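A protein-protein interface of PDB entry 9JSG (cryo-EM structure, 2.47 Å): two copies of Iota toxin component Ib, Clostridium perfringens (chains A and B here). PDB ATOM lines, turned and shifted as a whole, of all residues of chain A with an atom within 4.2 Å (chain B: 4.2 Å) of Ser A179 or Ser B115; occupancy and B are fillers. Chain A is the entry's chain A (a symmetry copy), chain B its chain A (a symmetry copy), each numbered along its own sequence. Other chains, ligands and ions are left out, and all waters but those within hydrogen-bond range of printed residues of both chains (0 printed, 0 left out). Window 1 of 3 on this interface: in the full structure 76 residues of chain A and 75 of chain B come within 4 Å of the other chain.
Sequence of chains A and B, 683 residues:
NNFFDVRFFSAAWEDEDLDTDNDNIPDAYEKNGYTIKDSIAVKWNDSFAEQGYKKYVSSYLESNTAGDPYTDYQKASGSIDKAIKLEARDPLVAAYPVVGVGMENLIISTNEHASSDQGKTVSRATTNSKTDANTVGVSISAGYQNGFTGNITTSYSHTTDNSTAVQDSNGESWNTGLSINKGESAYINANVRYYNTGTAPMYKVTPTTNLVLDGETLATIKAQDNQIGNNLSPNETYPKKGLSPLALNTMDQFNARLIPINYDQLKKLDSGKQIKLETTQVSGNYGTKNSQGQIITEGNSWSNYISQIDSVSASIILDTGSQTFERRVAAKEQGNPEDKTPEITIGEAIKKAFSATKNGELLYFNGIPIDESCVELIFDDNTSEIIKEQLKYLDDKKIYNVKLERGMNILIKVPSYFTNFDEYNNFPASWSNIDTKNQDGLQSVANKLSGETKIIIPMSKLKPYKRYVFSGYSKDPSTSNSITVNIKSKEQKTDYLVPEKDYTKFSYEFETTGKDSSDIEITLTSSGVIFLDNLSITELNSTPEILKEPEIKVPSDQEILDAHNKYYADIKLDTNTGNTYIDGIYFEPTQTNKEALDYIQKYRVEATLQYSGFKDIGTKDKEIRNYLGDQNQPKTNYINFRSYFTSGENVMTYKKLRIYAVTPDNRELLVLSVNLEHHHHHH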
ATOM      1  N   GLU A 112      24.560  20.026   6.468  1.00  0.00           N
ATOM      2  CA  GLU A 112      23.461  19.094   6.666  1.00  0.00           C
ATOM      3  C   GLU A 112      22.392  19.336   5.608  1.00  0.00           C
ATOM      4  O   GLU A 112      22.156  20.477   5.200  1.00  0.00           O
ATOM      5  CB  GLU A 112      22.861  19.223   8.069  1.00  0.00           C
ATOM      6  CG  GLU A 112      22.482  20.635   8.470  1.00  0.00           C
ATOM      7  CD  GLU A 112      22.184  20.767   9.954  1.00  0.00           C
ATOM      8  OE1 GLU A 112      22.894  20.141  10.770  1.00  0.00           O
ATOM      9  OE2 GLU A 112      21.237  21.500  10.306  1.00  0.00           O
ATOM     10  N   HIS A 113      21.763  18.255   5.156  1.00  0.00           N
ATOM     11  CA  HIS A 113      20.759  18.298   4.100  1.00  0.00           C
ATOM     12  C   HIS A 113      19.374  18.132   4.711  1.00  0.00           C
ATOM     13  O   HIS A 113      19.114  17.150   5.410  1.00  0.00           O
ATOM     14  CB  HIS A 113      21.020  17.202   3.063  1.00  0.00           C
ATOM     15  CG  HIS A 113      20.233  17.361   1.800  1.00  0.00           C
ATOM     16  ND1 HIS A 113      20.511  18.333   0.862  1.00  0.00           N
ATOM     17  CD2 HIS A 113      19.175  16.665   1.317  1.00  0.00           C
ATOM     18  CE1 HIS A 113      19.659  18.228  -0.142  1.00  0.00           C
ATOM     19  NE2 HIS A 113      18.838  17.226   0.109  1.00  0.00           N
ATOM     20  N   LEU A 178      16.257  14.924   7.698  1.00  0.00           N
ATOM     21  CA  LEU A 178      17.526  15.612   7.917  1.00  0.00           C
ATOM     22  C   LEU A 178      18.645  14.586   7.878  1.00  0.00           C
ATOM     23  O   LEU A 178      18.575  13.569   8.576  1.00  0.00           O
ATOM     24  CB  LEU A 178      17.522  16.359   9.249  1.00  0.00           C
ATOM     25  CG  LEU A 178      18.715  17.279   9.507  1.00  0.00           C
ATOM     26  CD1 LEU A 178      18.636  18.522   8.636  1.00  0.00           C
ATOM     27  CD2 LEU A 178      18.791  17.655  10.978  1.00  0.00           C
ATOM     28  N   SER A 179      19.669  14.847   7.071  1.00  0.00           N
ATOM     29  CA  SER A 179      20.809  13.952   6.929  1.00  0.00           C
ATOM     30  C   SER A 179      22.100  14.730   7.138  1.00  0.00           C
ATOM     31  O   SER A 179      22.175  15.930   6.860  1.00  0.00           O
ATOM     32  CB  SER A 179      20.826  13.275   5.554  1.00  0.00           C
ATOM     33  OG  SER A 179      20.588  14.212   4.520  1.00  0.00           O
ATOM     34  N   ILE A 180      23.121  14.028   7.632  1.00  0.00           N
ATOM     35  CA  ILE A 180      24.406  14.634   7.949  1.00  0.00           C
ATOM     36  C   ILE A 180      25.520  13.647   7.626  1.00  0.00           C
ATOM     37  O   ILE A 180      25.355  12.429   7.748  1.00  0.00           O
ATOM     38  CB  ILE A 180      24.473  15.082   9.431  1.00  0.00           C
ATOM     39  CG1 ILE A 180      25.723  15.928   9.692  1.00  0.00           C
ATOM     40  CG2 ILE A 180      24.429  13.882  10.364  1.00  0.00           C
ATOM     41  CD1 ILE A 180      25.859  17.114   8.766  1.00  0.00           C
ATOM     42  N   HIS B 113      27.198   8.262   6.771  1.00  0.00           N
ATOM     43  CA  HIS B 113      26.069   9.152   6.530  1.00  0.00           C
ATOM     44  C   HIS B 113      24.901   8.742   7.416  1.00  0.00           C
ATOM     45  O   HIS B 113      24.461   7.591   7.377  1.00  0.00           O
ATOM     46  CB  HIS B 113      25.659   9.115   5.055  1.00  0.00           C
ATOM     47  CG  HIS B 113      24.721  10.211   4.656  1.00  0.00           C
ATOM     48  ND1 HIS B 113      25.119  11.526   4.526  1.00  0.00           N
ATOM     49  CD2 HIS B 113      23.401  10.187   4.356  1.00  0.00           C
ATOM     50  CE1 HIS B 113      24.085  12.262   4.162  1.00  0.00           C
ATOM     51  NE2 HIS B 113      23.030  11.476   4.053  1.00  0.00           N
ATOM     52  N   ALA B 114      24.397   9.688   8.205  1.00  0.00           N
ATOM     53  CA  ALA B 114      23.289   9.448   9.117  1.00  0.00           C
ATOM     54  C   ALA B 114      22.099  10.304   8.709  1.00  0.00           C
ATOM     55  O   ALA B 114      22.257  11.485   8.379  1.00  0.00           O
ATOM     56  CB  ALA B 114      23.684   9.754  10.564  1.00  0.00           C
ATOM     57  N   SER B 115      20.907   9.709   8.729  1.00  0.00           N
ATOM     58  CA  SER B 115      19.696  10.396   8.309  1.00  0.00           C
ATOM     59  C   SER B 115      18.560  10.080   9.274  1.00  0.00           C
ATOM     60  O   SER B 115      18.504   9.000   9.867  1.00  0.00           O
ATOM     61  CB  SER B 115      19.292  10.007   6.880  1.00  0.00           C
ATOM     62  OG  SER B 115      19.591   8.647   6.621  1.00  0.00           O
ATOM     63  N   SER B 116      17.646  11.037   9.412  1.00  0.00           N
ATOM     64  CA  SER B 116      16.464  10.877  10.246  1.00  0.00           C
ATOM     65  C   SER B 116      15.261  11.435   9.497  1.00  0.00           C
ATOM     66  O   SER B 116      15.370  12.457   8.814  1.00  0.00           O
ATOM     67  CB  SER B 116      16.626  11.586  11.596  1.00  0.00           C
ATOM     68  OG  SER B 116      17.063  12.922  11.419  1.00  0.00           O
ATOM     69  N   THR B 176      15.219   6.147  11.210  1.00  0.00           N
ATOM     70  CA  THR B 176      16.631   6.478  11.343  1.00  0.00           C
ATOM     71  C   THR B 176      17.441   5.550  10.450  1.00  0.00           C
ATOM     72  O   THR B 176      17.140   4.357  10.347  1.00  0.00           O
ATOM     73  CB  THR B 176      17.113   6.353  12.796  1.00  0.00           C
ATOM     74  OG1 THR B 176      16.678   5.103  13.343  1.00  0.00           O
ATOM     75  CG2 THR B 176      16.566   7.493  13.642  1.00  0.00           C
ATOM     76  N   GLY B 177      18.469   6.099   9.804  1.00  0.00           N
ATOM     77  CA  GLY B 177      19.274   5.322   8.886  1.00  0.00           C
ATOM     78  C   GLY B 177      20.737   5.703   8.972  1.00  0.00           C
ATOM     79  O   GLY B 177      21.093   6.852   9.245  1.00  0.00           O
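N of Ser B116 is in hydrogen-bond range of O of Leu A178 (2.8 Å).
The backbone carbonyl oxygen (O) of Ile A180 sits at hydrogen-bond distance from a ring nitrogen (ND1) of His B113 (3.4 Å).
The backbone NH of Ile A180 is in hydrogen-bond range of the backbone carbonyl oxygen of Ala B114 (2.8 Å).
O of His A113 lies within hydrogen-bond range of N of Ser A179 (2.9 Å).
N of Gly B177 lies within hydrogen-bond range of O of Ser B115 (2.9 Å).
Among the printed residues, merely in contact across the chains: Ser A179 with Ala B114 (3.2 Å), Ser A179 with His B113 (3.2 Å), Leu A178 with Ser B115 (3.4 Å) and Ser A179 with Ser B115 (3.8 Å).
Of the printed residues of chain B, Leu A178 touches Ser B115 (3.4 Å) and Ser B116 (2.8 Å).
Ser A179 touches three residues of chain B.
Of the printed residues of chain B, Ile A180 touches His B113 (3.4 Å) and Ala B114 (2.8 Å).
Printed residues of chain A within 4 Å of His B113: Ser A179 and Ile A180.
Printed residues of chain A within 4 Å of Ala B114: Ser A179 (3.2 Å) and Ile A180 (2.8 Å).
Printed residues of chain A within 4 Å of Ser B115: Leu A178 and Ser A179.
Of the printed residues of chain A, Ser B116 touches Leu A178.
The nearest printed residue of chain B that does not touch Ser A179 is Ser B116 (4.9 Å).
Of the 5 printed residues of chain A, 3 touch a printed residue of chain B.
Hydrophobic or aromatic side chains of chain A within 4 Å of the printed part of chain B: Ile A180.
Of the 6 printed residues of chain B, 4 touch a printed residue of chain A.
Among the printed residues, no Asp or Glu carboxylate lies within 4 Å of a Lys or Arg side-chain nitrogen of the other chain.
Position printed for both chains: 113.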
